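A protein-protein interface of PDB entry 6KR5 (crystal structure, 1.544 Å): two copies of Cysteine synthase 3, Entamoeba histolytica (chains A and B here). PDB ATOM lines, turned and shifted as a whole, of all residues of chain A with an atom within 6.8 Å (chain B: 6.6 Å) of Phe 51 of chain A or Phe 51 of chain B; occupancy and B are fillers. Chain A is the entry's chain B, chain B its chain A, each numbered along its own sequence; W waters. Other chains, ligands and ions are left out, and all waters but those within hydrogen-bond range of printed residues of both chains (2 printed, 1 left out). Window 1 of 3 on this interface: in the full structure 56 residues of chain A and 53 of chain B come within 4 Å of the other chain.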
ATOM      1  N   ASN A   7     -11.243  18.186  11.769  1.00  0.00           N
ATOM      2  CA  ASN A   7     -12.319  17.330  12.232  1.00  0.00           C
ATOM      3  C   ASN A   7     -12.370  16.022  11.447  1.00  0.00           C
ATOM      4  O   ASN A   7     -11.935  15.933  10.296  1.00  0.00           O
ATOM      5  CB  ASN A   7     -13.662  18.055  12.128  1.00  0.00           C
ATOM      6  CG  ASN A   7     -14.275  18.341  13.480  1.00  0.00           C
ATOM      7  OD1 ASN A   7     -14.105  17.572  14.427  1.00  0.00           O
ATOM      8  ND2 ASN A   7     -14.996  19.452  13.582  1.00  0.00           N
ATOM      9  N   ILE A  17     -32.467  18.973  10.646  1.00  0.00           N
ATOM     10  CA  ILE A  17     -31.506  19.928  11.190  1.00  0.00           C
ATOM     11  C   ILE A  17     -31.525  19.928  12.713  1.00  0.00           C
ATOM     12  O   ILE A  17     -30.512  20.249  13.342  1.00  0.00           O
ATOM     13  CB  ILE A  17     -31.757  21.332  10.595  1.00  0.00           C
ATOM     14  CG1 ILE A  17     -30.558  22.251  10.842  1.00  0.00           C
ATOM     15  CG2 ILE A  17     -33.059  21.961  11.113  1.00  0.00           C
ATOM     16  CD1 ILE A  17     -29.297  21.771  10.174  1.00  0.00           C
ATOM     17  N   THR A  20     -28.768  18.058  14.558  1.00  0.00           N
ATOM     18  CA  THR A  20     -27.416  18.610  14.618  1.00  0.00           C
ATOM     19  C   THR A  20     -27.223  19.589  15.766  1.00  0.00           C
ATOM     20  O   THR A  20     -26.108  20.087  15.946  1.00  0.00           O
ATOM     21  CB  THR A  20     -27.023  19.327  13.315  1.00  0.00           C
ATOM     22  OG1 THR A  20     -27.738  20.563  13.190  1.00  0.00           O
ATOM     23  CG2 THR A  20     -27.267  18.460  12.089  1.00  0.00           C
ATOM     24  N   ILE A  21     -28.270  19.874  16.539  1.00  0.00           N
ATOM     25  CA  ILE A  21     -28.145  20.816  17.640  1.00  0.00           C
ATOM     26  C   ILE A  21     -27.266  20.225  18.729  1.00  0.00           C
ATOM     27  O   ILE A  21     -27.359  19.029  19.053  1.00  0.00           O
ATOM     28  CB  ILE A  21     -29.535  21.169  18.190  1.00  0.00           C
ATOM     29  CG1 ILE A  21     -30.311  21.965  17.158  1.00  0.00           C
ATOM     30  CG2 ILE A  21     -29.437  21.952  19.509  1.00  0.00           C
ATOM     31  CD1 ILE A  21     -31.756  22.216  17.584  1.00  0.00           C
ATOM     32  N   GLY A  22     -26.423  21.072  19.316  1.00  0.00           N
ATOM     33  CA  GLY A  22     -25.541  20.644  20.379  1.00  0.00           C
ATOM     34  C   GLY A  22     -24.294  19.921  19.891  1.00  0.00           C
ATOM     35  O   GLY A  22     -23.850  20.038  18.735  1.00  0.00           O
ATOM     36  N   GLY A  23     -23.709  19.170  20.819  1.00  0.00           N
ATOM     37  CA  GLY A  23     -22.414  18.551  20.555  1.00  0.00           C
ATOM     38  C   GLY A  23     -21.385  19.530  20.039  1.00  0.00           C
ATOM     39  O   GLY A  23     -20.661  19.226  19.084  1.00  0.00           O
ATOM     40  N   THR A  24     -21.319  20.715  20.645  1.00  0.00           N
ATOM     41  CA  THR A  24     -20.467  21.794  20.147  1.00  0.00           C
ATOM     42  C   THR A  24     -19.022  21.647  20.616  1.00  0.00           C
ATOM     43  O   THR A  24     -18.748  21.003  21.630  1.00  0.00           O
ATOM     44  CB  THR A  24     -21.015  23.138  20.611  1.00  0.00           C
ATOM     45  OG1 THR A  24     -21.093  23.147  22.037  1.00  0.00           O
ATOM     46  CG2 THR A  24     -22.407  23.387  20.014  1.00  0.00           C
ATOM     47  N   PRO A  25     -18.073  22.234  19.886  1.00  0.00           N
ATOM     48  CA  PRO A  25     -16.658  21.999  20.198  1.00  0.00           C
ATOM     49  C   PRO A  25     -16.208  22.743  21.436  1.00  0.00           C
ATOM     50  O   PRO A  25     -16.693  23.833  21.745  1.00  0.00           O
ATOM     51  CB  PRO A  25     -15.924  22.537  18.965  1.00  0.00           C
ATOM     52  CG  PRO A  25     -16.967  22.831  17.949  1.00  0.00           C
ATOM     53  CD  PRO A  25     -18.238  23.060  18.684  1.00  0.00           C
ATOM     54  N   VAL A  27     -12.641  24.216  22.826  1.00  0.00           N
ATOM     55  CA  VAL A  27     -11.404  24.635  22.163  1.00  0.00           C
ATOM     56  C   VAL A  27     -10.495  25.362  23.149  1.00  0.00           C
ATOM     57  O   VAL A  27     -10.951  26.198  23.937  1.00  0.00           O
ATOM     58  CB  VAL A  27     -11.715  25.542  20.950  1.00  0.00           C
ATOM     59  CG1 VAL A  27     -10.429  25.946  20.204  1.00  0.00           C
ATOM     60  CG2 VAL A  27     -12.699  24.846  20.012  1.00  0.00           C
ATOM     61  N   LEU A  48     -18.055  26.514  22.058  1.00  0.00           N
ATOM     62  CA  LEU A  48     -18.482  27.377  20.954  1.00  0.00           C
ATOM     63  C   LEU A  48     -19.916  27.049  20.554  1.00  0.00           C
ATOM     64  O   LEU A  48     -20.163  26.237  19.655  1.00  0.00           O
ATOM     65  CB  LEU A  48     -17.523  27.231  19.783  1.00  0.00           C
ATOM     66  CG  LEU A  48     -16.082  27.444  20.218  1.00  0.00           C
ATOM     67  CD1 LEU A  48     -15.184  27.322  19.005  1.00  0.00           C
ATOM     68  CD2 LEU A  48     -15.927  28.800  20.823  1.00  0.00           C
ATOM     69  N   GLU A  49     -20.869  27.738  21.191  1.00  0.00           N
ATOM     70  CA  GLU A  49     -22.269  27.521  20.857  1.00  0.00           C
ATOM     71  C   GLU A  49     -22.621  28.101  19.496  1.00  0.00           C
ATOM     72  O   GLU A  49     -23.723  27.856  18.989  1.00  0.00           O
ATOM     73  CB  GLU A  49     -23.153  28.085  21.971  1.00  0.00           C
ATOM     74  CG  GLU A  49     -22.973  27.292  23.268  1.00  0.00           C
ATOM     75  CD  GLU A  49     -23.429  25.846  23.104  1.00  0.00           C
ATOM     76  OE1 GLU A  49     -24.603  25.668  22.714  1.00  0.00           O
ATOM     77  OE2 GLU A  49     -22.635  24.907  23.364  1.00  0.00           O
ATOM     78  N   CYS A  50     -21.702  28.833  18.873  1.00  0.00           N
ATOM     79  CA  CYS A  50     -21.892  29.246  17.494  1.00  0.00           C
ATOM     80  C   CYS A  50     -21.944  28.062  16.534  1.00  0.00           C
ATOM     81  O   CYS A  50     -22.378  28.228  15.385  1.00  0.00           O
ATOM     82  CB  CYS A  50     -20.764  30.186  17.101  1.00  0.00           C
ATOM     83  SG  CYS A  50     -20.912  30.804  15.445  1.00  0.00           S
ATOM     84  N   PHE A  51     -21.519  26.874  16.971  1.00  0.00           N
ATOM     85  CA  PHE A  51     -21.551  25.705  16.101  1.00  0.00           C
ATOM     86  C   PHE A  51     -22.936  25.079  15.984  1.00  0.00           C
ATOM     87  O   PHE A  51     -23.112  24.158  15.181  1.00  0.00           O
ATOM     88  CB  PHE A  51     -20.533  24.666  16.575  1.00  0.00           C
ATOM     89  CG  PHE A  51     -19.153  24.890  16.025  1.00  0.00           C
ATOM     90  CD1 PHE A  51     -18.372  25.912  16.509  1.00  0.00           C
ATOM     91  CD2 PHE A  51     -18.646  24.069  15.037  1.00  0.00           C
ATOM     92  CE1 PHE A  51     -17.093  26.119  16.003  1.00  0.00           C
ATOM     93  CE2 PHE A  51     -17.376  24.280  14.530  1.00  0.00           C
ATOM     94  CZ  PHE A  51     -16.608  25.298  15.022  1.00  0.00           C
ATOM     95  N   ASN A  52     -23.923  25.541  16.752  1.00  0.00           N
ATOM     96  CA  ASN A  52     -25.294  25.111  16.513  1.00  0.00           C
ATOM     97  C   ASN A  52     -25.745  25.546  15.117  1.00  0.00           C
ATOM     98  O   ASN A  52     -25.200  26.501  14.547  1.00  0.00           O
ATOM     99  CB  ASN A  52     -26.206  25.690  17.590  1.00  0.00           C
ATOM    100  CG  ASN A  52     -26.071  24.954  18.909  1.00  0.00           C
ATOM    101  OD1 ASN A  52     -26.461  23.792  19.019  1.00  0.00           O
ATOM    102  ND2 ASN A  52     -25.495  25.614  19.909  1.00  0.00           N
ATOM    103  N   PRO A  53     -26.727  24.851  14.526  1.00  0.00           N
ATOM    104  CA  PRO A  53     -27.114  25.171  13.134  1.00  0.00           C
ATOM    105  C   PRO A  53     -27.526  26.617  12.907  1.00  0.00           C
ATOM    106  O   PRO A  53     -27.225  27.173  11.838  1.00  0.00           O
ATOM    107  CB  PRO A  53     -28.276  24.202  12.857  1.00  0.00           C
ATOM    108  CG  PRO A  53     -28.684  23.653  14.215  1.00  0.00           C
ATOM    109  CD  PRO A  53     -27.426  23.659  15.034  1.00  0.00           C
ATOM    110  N   MET A  54     -28.210  27.253  13.863  1.00  0.00           N
ATOM    111  CA  MET A  54     -28.477  28.680  13.755  1.00  0.00           C
ATOM    112  C   MET A  54     -27.602  29.485  14.713  1.00  0.00           C
ATOM    113  O   MET A  54     -27.914  30.635  15.038  1.00  0.00           O
ATOM    114  CB  MET A  54     -29.966  28.974  13.942  1.00  0.00           C
ATOM    115  CG  MET A  54     -30.784  28.742  12.658  1.00  0.00           C
ATOM    116  SD  MET A  54     -30.119  29.534  11.164  1.00  0.00           S
ATOM    117  CE  MET A  54     -30.108  31.240  11.703  1.00  0.00           C
ATOM    118  N   SER A  55     -26.489  28.891  15.141  1.00  0.00           N
ATOM    119  CA  SER A  55     -25.300  29.618  15.590  1.00  0.00           C
ATOM    120  C   SER A  55     -25.475  30.323  16.928  1.00  0.00           C
ATOM    121  O   SER A  55     -24.779  31.306  17.209  1.00  0.00           O
ATOM    122  CB  SER A  55     -24.837  30.613  14.525  1.00  0.00           C
ATOM    123  OG  SER A  55     -24.595  29.911  13.319  1.00  0.00           O
ATOM    124  N   SER A  56     -26.355  29.825  17.791  1.00  0.00           N
ATOM    125  CA  SER A  56     -26.341  30.300  19.165  1.00  0.00           C
ATOM    126  C   SER A  56     -26.830  29.207  20.095  1.00  0.00           C
ATOM    127  O   SER A  56     -27.443  28.225  19.677  1.00  0.00           O
ATOM    128  CB  SER A  56     -27.191  31.558  19.363  1.00  0.00           C
ATOM    129  OG  SER A  56     -28.530  31.219  19.714  1.00  0.00           O
ATOM    130  N   ASP A  59     -30.456  27.697  20.092  1.00  0.00           N
ATOM    131  CA  ASP A  59     -30.914  26.519  19.357  1.00  0.00           C
ATOM    132  C   ASP A  59     -31.338  25.424  20.325  1.00  0.00           C
ATOM    133  O   ASP A  59     -32.355  24.749  20.120  1.00  0.00           O
ATOM    134  CB  ASP A  59     -29.805  25.972  18.454  1.00  0.00           C
ATOM    135  CG  ASP A  59     -29.599  26.774  17.189  1.00  0.00           C
ATOM    136  OD1 ASP A  59     -29.815  27.998  17.191  1.00  0.00           O
ATOM    137  OD2 ASP A  59     -29.188  26.151  16.184  1.00  0.00           O
ATOM    138  N   LEU A 306     -19.354  30.312  25.174  1.00  0.00           N
ATOM    139  CA  LEU A 306     -19.422  31.406  24.202  1.00  0.00           C
ATOM    140  C   LEU A 306     -20.768  31.314  23.490  1.00  0.00           C
ATOM    141  O   LEU A 306     -20.934  30.467  22.601  1.00  0.00           O
ATOM    142  CB  LEU A 306     -18.267  31.333  23.195  1.00  0.00           C
ATOM    143  CG  LEU A 306     -16.845  31.242  23.777  1.00  0.00           C
ATOM    144  CD1 LEU A 306     -15.827  31.627  22.702  1.00  0.00           C
ATOM    145  CD2 LEU A 306     -16.681  32.111  24.980  1.00  0.00           C
ATOM    146  N   ASN B   7     -27.377  16.055  18.810  1.00  0.00           N
ATOM    147  CA  ASN B   7     -25.947  15.749  18.651  1.00  0.00           C
ATOM    148  C   ASN B   7     -25.355  15.130  19.914  1.00  0.00           C
ATOM    149  O   ASN B   7     -25.791  15.388  21.017  1.00  0.00           O
ATOM    150  CB  ASN B   7     -25.188  16.947  18.112  1.00  0.00           C
ATOM    151  CG  ASN B   7     -24.315  16.594  16.943  1.00  0.00           C
ATOM    152  OD1 ASN B   7     -23.927  15.453  16.792  1.00  0.00           O
ATOM    153  ND2 ASN B   7     -24.062  17.565  16.088  1.00  0.00           N
ATOM    154  N   ILE B  17      -8.922  26.759  16.775  1.00  0.00           N
ATOM    155  CA  ILE B  17     -10.148  26.771  15.986  1.00  0.00           C
ATOM    156  C   ILE B  17      -9.972  26.052  14.652  1.00  0.00           C
ATOM    157  O   ILE B  17     -10.946  25.551  14.082  1.00  0.00           O
ATOM    158  CB  ILE B  17     -10.626  28.227  15.800  1.00  0.00           C
ATOM    159  CG1 ILE B  17     -12.061  28.282  15.272  1.00  0.00           C
ATOM    160  CG2 ILE B  17      -9.705  29.000  14.861  1.00  0.00           C
ATOM    161  CD1 ILE B  17     -13.096  27.777  16.236  1.00  0.00           C
ATOM    162  N   THR B  20     -11.320  22.537  14.304  1.00  0.00           N
ATOM    163  CA  THR B  20     -12.761  22.347  14.155  1.00  0.00           C
ATOM    164  C   THR B  20     -13.221  22.404  12.702  1.00  0.00           C
ATOM    165  O   THR B  20     -14.410  22.190  12.435  1.00  0.00           O
ATOM    166  CB  THR B  20     -13.548  23.395  14.968  1.00  0.00           C
ATOM    167  OG1 THR B  20     -13.429  24.685  14.355  1.00  0.00           O
ATOM    168  CG2 THR B  20     -13.079  23.447  16.420  1.00  0.00           C
ATOM    169  N   ILE B  21     -12.315  22.671  11.758  1.00  0.00           N
ATOM    170  CA  ILE B  21     -12.694  22.746  10.356  1.00  0.00           C
ATOM    171  C   ILE B  21     -13.073  21.364   9.833  1.00  0.00           C
ATOM    172  O   ILE B  21     -12.468  20.348  10.205  1.00  0.00           O
ATOM    173  CB  ILE B  21     -11.546  23.364   9.537  1.00  0.00           C
ATOM    174  CG1 ILE B  21     -11.390  24.845   9.916  1.00  0.00           C
ATOM    175  CG2 ILE B  21     -11.800  23.175   8.039  1.00  0.00           C
ATOM    176  CD1 ILE B  21     -10.133  25.507   9.327  1.00  0.00           C
ATOM    177  N   GLY B  22     -14.101  21.319   8.976  1.00  0.00           N
ATOM    178  CA  GLY B  22     -14.508  20.079   8.343  1.00  0.00           C
ATOM    179  C   GLY B  22     -15.337  19.193   9.256  1.00  0.00           C
ATOM    180  O   GLY B  22     -15.853  19.617  10.295  1.00  0.00           O
ATOM    181  N   GLY B  23     -15.443  17.931   8.855  1.00  0.00           N
ATOM    182  CA  GLY B  23     -16.324  17.007   9.559  1.00  0.00           C
ATOM    183  C   GLY B  23     -17.732  17.537   9.698  1.00  0.00           C
ATOM    184  O   GLY B  23     -18.333  17.445  10.776  1.00  0.00           O
ATOM    185  N   THR B  24     -18.268  18.106   8.627  1.00  0.00           N
ATOM    186  CA  THR B  24     -19.547  18.798   8.688  1.00  0.00           C
ATOM    187  C   THR B  24     -20.708  17.824   8.545  1.00  0.00           C
ATOM    188  O   THR B  24     -20.555  16.735   7.990  1.00  0.00           O
ATOM    189  CB  THR B  24     -19.618  19.847   7.584  1.00  0.00           C
ATOM    190  OG1 THR B  24     -19.389  19.208   6.326  1.00  0.00           O
ATOM    191  CG2 THR B  24     -18.582  20.936   7.817  1.00  0.00           C
ATOM    192  N   PRO B  25     -21.892  18.201   9.032  1.00  0.00           N
ATOM    193  CA  PRO B  25     -23.024  17.267   9.029  1.00  0.00           C
ATOM    194  C   PRO B  25     -23.585  17.015   7.644  1.00  0.00           C
ATOM    195  O   PRO B  25     -23.667  17.913   6.802  1.00  0.00           O
ATOM    196  CB  PRO B  25     -24.073  17.978   9.891  1.00  0.00           C
ATOM    197  CG  PRO B  25     -23.353  19.049  10.614  1.00  0.00           C
ATOM    198  CD  PRO B  25     -22.223  19.457   9.718  1.00  0.00           C
ATOM    199  N   VAL B  27     -27.201  15.825   6.185  1.00  0.00           N
ATOM    200  CA  VAL B  27     -28.566  15.894   6.711  1.00  0.00           C
ATOM    201  C   VAL B  27     -29.570  15.537   5.619  1.00  0.00           C
ATOM    202  O   VAL B  27     -29.445  15.992   4.476  1.00  0.00           O
ATOM    203  CB  VAL B  27     -28.871  17.298   7.280  1.00  0.00           C
ATOM    204  CG1 VAL B  27     -30.297  17.364   7.905  1.00  0.00           C
ATOM    205  CG2 VAL B  27     -27.800  17.700   8.298  1.00  0.00           C
ATOM    206  N   LEU B  48     -23.572  20.329   5.107  1.00  0.00           N
ATOM    207  CA  LEU B  48     -23.754  21.689   5.608  1.00  0.00           C
ATOM    208  C   LEU B  48     -22.395  22.301   5.923  1.00  0.00           C
ATOM    209  O   LEU B  48     -21.891  22.227   7.046  1.00  0.00           O
ATOM    210  CB  LEU B  48     -24.670  21.673   6.824  1.00  0.00           C
ATOM    211  CG  LEU B  48     -26.030  21.027   6.537  1.00  0.00           C
ATOM    212  CD1 LEU B  48     -26.924  21.184   7.749  1.00  0.00           C
ATOM    213  CD2 LEU B  48     -26.662  21.654   5.336  1.00  0.00           C
ATOM    214  N   GLU B  49     -21.798  22.924   4.911  1.00  0.00           N
ATOM    215  CA  GLU B  49     -20.500  23.556   5.107  1.00  0.00           C
ATOM    216  C   GLU B  49     -20.586  24.813   5.961  1.00  0.00           C
ATOM    217  O   GLU B  49     -19.546  25.336   6.377  1.00  0.00           O
ATOM    218  CB  GLU B  49     -19.870  23.845   3.747  1.00  0.00           C
ATOM    219  CG  GLU B  49     -19.441  22.557   3.035  1.00  0.00           C
ATOM    220  CD  GLU B  49     -18.408  21.779   3.834  1.00  0.00           C
ATOM    221  OE1 GLU B  49     -17.354  22.368   4.141  1.00  0.00           O
ATOM    222  OE2 GLU B  49     -18.648  20.594   4.144  1.00  0.00           O
ATOM    223  N   CYS B  50     -21.796  25.292   6.261  1.00  0.00           N
ATOM    224  CA  CYS B  50     -21.960  26.369   7.224  1.00  0.00           C
ATOM    225  C   CYS B  50     -21.508  25.975   8.628  1.00  0.00           C
ATOM    226  O   CYS B  50     -21.333  26.860   9.479  1.00  0.00           O
ATOM    227  CB  CYS B  50     -23.428  26.804   7.254  1.00  0.00           C
ATOM    228  SG  CYS B  50     -23.727  28.250   8.254  1.00  0.00           S
ATOM    229  N   PHE B  51     -21.317  24.678   8.894  1.00  0.00           N
ATOM    230  CA  PHE B  51     -20.860  24.233  10.204  1.00  0.00           C
ATOM    231  C   PHE B  51     -19.368  24.447  10.416  1.00  0.00           C
ATOM    232  O   PHE B  51     -18.886  24.242  11.536  1.00  0.00           O
ATOM    233  CB  PHE B  51     -21.217  22.755  10.424  1.00  0.00           C
ATOM    234  CG  PHE B  51     -22.602  22.543  10.999  1.00  0.00           C
ATOM    235  CD1 PHE B  51     -23.729  22.771  10.229  1.00  0.00           C
ATOM    236  CD2 PHE B  51     -22.764  22.118  12.302  1.00  0.00           C
ATOM    237  CE1 PHE B  51     -25.009  22.565  10.753  1.00  0.00           C
ATOM    238  CE2 PHE B  51     -24.038  21.912  12.832  1.00  0.00           C
ATOM    239  CZ  PHE B  51     -25.153  22.142  12.057  1.00  0.00           C
ATOM    240  N   ASN B  52     -18.620  24.869   9.389  1.00  0.00           N
ATOM    241  CA  ASN B  52     -17.237  25.263   9.616  1.00  0.00           C
ATOM    242  C   ASN B  52     -17.197  26.474  10.547  1.00  0.00           C
ATOM    243  O   ASN B  52     -18.178  27.211  10.658  1.00  0.00           O
ATOM    244  CB  ASN B  52     -16.564  25.580   8.285  1.00  0.00           C
ATOM    245  CG  ASN B  52     -16.178  24.334   7.535  1.00  0.00           C
ATOM    246  OD1 ASN B  52     -15.266  23.616   7.941  1.00  0.00           O
ATOM    247  ND2 ASN B  52     -16.882  24.050   6.454  1.00  0.00           N
ATOM    248  N   PRO B  53     -16.071  26.705  11.242  1.00  0.00           N
ATOM    249  CA  PRO B  53     -16.078  27.771  12.263  1.00  0.00           C
ATOM    250  C   PRO B  53     -16.417  29.149  11.721  1.00  0.00           C
ATOM    251  O   PRO B  53     -17.107  29.916  12.415  1.00  0.00           O
ATOM    252  CB  PRO B  53     -14.656  27.724  12.850  1.00  0.00           C
ATOM    253  CG  PRO B  53     -13.854  26.878  11.889  1.00  0.00           C
ATOM    254  CD  PRO B  53     -14.834  25.912  11.286  1.00  0.00           C
ATOM    255  N   MET B  54     -15.968  29.502  10.512  1.00  0.00           N
ATOM    256  CA  MET B  54     -16.402  30.749   9.896  1.00  0.00           C
ATOM    257  C   MET B  54     -17.436  30.507   8.807  1.00  0.00           C
ATOM    258  O   MET B  54     -17.610  31.345   7.915  1.00  0.00           O
ATOM    259  CB  MET B  54     -15.206  31.551   9.375  1.00  0.00           C
ATOM    260  CG  MET B  54     -14.532  32.396  10.470  1.00  0.00           C
ATOM    261  SD  MET B  54     -15.674  33.399  11.445  1.00  0.00           S
ATOM    262  CE  MET B  54     -16.283  34.506  10.179  1.00  0.00           C
ATOM    263  N   SER B  55     -18.110  29.356   8.870  1.00  0.00           N
ATOM    264  CA  SER B  55     -19.421  29.130   8.267  1.00  0.00           C
ATOM    265  C   SER B  55     -19.396  29.078   6.748  1.00  0.00           C
ATOM    266  O   SER B  55     -20.412  29.365   6.113  1.00  0.00           O
ATOM    267  CB  SER B  55     -20.435  30.182   8.726  1.00  0.00           C
ATOM    268  OG  SER B  55     -20.583  30.114  10.132  1.00  0.00           O
ATOM    269  N   SER B  56     -18.282  28.678   6.135  1.00  0.00           N
ATOM    270  CA  SER B  56     -18.342  28.361   4.716  1.00  0.00           C
ATOM    271  C   SER B  56     -17.316  27.295   4.380  1.00  0.00           C
ATOM    272  O   SER B  56     -16.385  27.024   5.139  1.00  0.00           O
ATOM    273  CB  SER B  56     -18.147  29.606   3.839  1.00  0.00           C
ATOM    274  OG  SER B  56     -16.773  29.783   3.483  1.00  0.00           O
ATOM    275  N   ASP B  59     -13.379  27.731   4.623  1.00  0.00           N
ATOM    276  CA  ASP B  59     -12.534  27.429   5.776  1.00  0.00           C
ATOM    277  C   ASP B  59     -11.540  26.335   5.416  1.00  0.00           C
ATOM    278  O   ASP B  59     -10.350  26.418   5.754  1.00  0.00           O
ATOM    279  CB  ASP B  59     -13.384  26.987   6.970  1.00  0.00           C
ATOM    280  CG  ASP B  59     -14.069  28.136   7.661  1.00  0.00           C
ATOM    281  OD1 ASP B  59     -14.284  29.182   7.017  1.00  0.00           O
ATOM    282  OD2 ASP B  59     -14.377  27.990   8.862  1.00  0.00           O
ATOM    283  N   CYS B 309     -24.163  29.825   4.618  1.00  0.00           N
ATOM    284  CA  CYS B 309     -25.453  30.112   5.235  1.00  0.00           C
ATOM    285  C   CYS B 309     -26.090  31.363   4.645  1.00  0.00           C
ATOM    286  O   CYS B 309     -25.423  32.248   4.106  1.00  0.00           O
ATOM    287  CB  CYS B 309     -25.300  30.300   6.748  1.00  0.00           C
ATOM    288  SG  CYS B 309     -25.607  28.825   7.757  1.00  0.00           S
HETATM  289  O   HOH W   1     -18.354  28.964  14.633  1.00  0.00           O
HETATM  290  O   HOH W   2     -26.945  17.983  21.646  1.00  0.00           O
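Phe 51 of chain B touches just these residues of chain A: Thr 20 (3.2 Å), Phe 51 (3.4 Å) and Pro 53 (3.8 Å).
Of the printed residues of chain A, Ile 21 of chain B touches Asn 7 (2.9 Å).
Of the printed residues of chain A, Pro 53 of chain B touches Phe 51 (3.7 Å).
Of the printed residues of chain A, Pro 25 of chain B touches Thr 20.
Of the printed residues of chain A, Leu 48 of chain B touches Ile 17 (3.4 Å).
Printed residues of chain B within 4 Å of Thr 20 of chain A: Asn 7 (3.3 Å), Pro 25 (3.9 Å), Val 27 (3.9 Å) and Phe 51 (3.2 Å).
The nearest residue of chain B that does not touch Phe 51 of chain A is Ile 17 of chain B (4.3 Å).
The side-chain amide nitrogen of Asn 7 of chain B is in hydrogen-bond range of the backbone carbonyl oxygen of Thr 20 of chain A.
The backbone NH (N) of Asn 7 of chain B sits at hydrogen-bond distance from the backbone carbonyl oxygen (O) of Ile 21 of chain A (3.0 Å).
O of Thr 20 of chain B lies within hydrogen-bond range of ND2 of Asn 7 of chain A, at 3.0 Å.
The backbone carbonyl oxygen (O) of Ile 21 of chain B is in hydrogen-bond range of the backbone NH (N) of Asn 7 of chain A (2.9 Å).
The backbone carbonyl oxygen of Gly 22 of chain B lies close to the side-chain amide nitrogen of Asn 7 of chain A.
Water W1 lies within hydrogen-bond range of O of Pro 53 of chain B and SG of Cys 50 of chain A.
Water W2 lies within hydrogen-bond range of the backbone carbonyl oxygen (O) of Ile 21 of chain A and the backbone carbonyl oxygen (O) of Asn 7 of chain B.
Along chain A the printed residues that touch a printed residue of chain B span positions 7 to 53.
Among the printed residues, no Asp or Glu carboxylate lies within 4 Å of a Lys or Arg side-chain nitrogen of the other chain.
Among the printed residues, pairs that only touch across the chains: Asn 7 of chain A with Gly 23 of chain B (3.7 Å), Ile 17 of chain A with Val 27 of chain B (3.8 Å), Ile 17 of chain A with Leu 48 of chain B (3.4 Å), Thr 20 of chain A with Pro 25 of chain B (3.9 Å), Thr 20 of chain A with Val 27 of chain B (3.9 Å), Thr 20 of chain A with Phe 51 of chain B (3.2 Å), Gly 22 of chain A with Asn 7 of chain B (3.4 Å), Gly 23 of chain A with Asn 7 of chain B (3.8 Å), Pro 25 of chain A with Thr 20 of chain B (3.9 Å), Val 27 of chain A with Ile 17 of chain B (3.8 Å), Val 27 of chain A with Thr 20 of chain B (3.9 Å), Leu 48 of chain A with Ile 17 of chain B (3.5 Å), Phe 51 of chain A with Thr 20 of chain B (3.3 Å), Phe 51 of chain A with Phe 51 of chain B (3.4 Å), Phe 51 of chain A with Pro 53 of chain B (3.7 Å) and Pro 53 of chain A with Phe 51 of chain B (3.8 Å).
The backbone carbonyl oxygen (O) of Ile 17 of chain B is in hydrogen-bond range of the side-chain hydroxyl (OG1) of Thr 20 of chain B (2.6 Å).
OD1 of Asn 52 of chain B sits at hydrogen-bond distance from N of Gly 22 of chain B (2.8 Å).
The backbone NH of Leu 48 of chain B sits at hydrogen-bond distance from the backbone carbonyl oxygen of Pro 25 of chain B (3.0 Å).
OD1 of Asn 52 of chain A sits at hydrogen-bond distance from N of Gly 22 of chain A (2.7 Å).
O of Pro 25 of chain A is in hydrogen-bond range of N of Leu 48 of chain A.
The side-chain sulfur of Cys 50 of chain B forms a disulfide with the side-chain sulfur of Cys 309 of chain B (2.0 Å).
Asn 7 of chain A touches Gly 23 of chain B, and with the chains exchanged Gly 23 of chain A touches Asn 7 of chain B.
Ile 17 of chain A touches Leu 48 of chain B, and with the chains exchanged Leu 48 of chain A touches Ile 17 of chain B.
Thr 20 of chain A touches Val 27 of chain B, and with the chains exchanged Val 27 of chain A touches Thr 20 of chain B.
Phe 51 of chain B touches its own counterpart, Phe 51 of chain A.
Positions printed for both chains: 7, 17, 20, 21, 22, 23, 24, 25, 27, 48, 49, 50, 51, 52, 53, 54, 55, 56 and 59.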
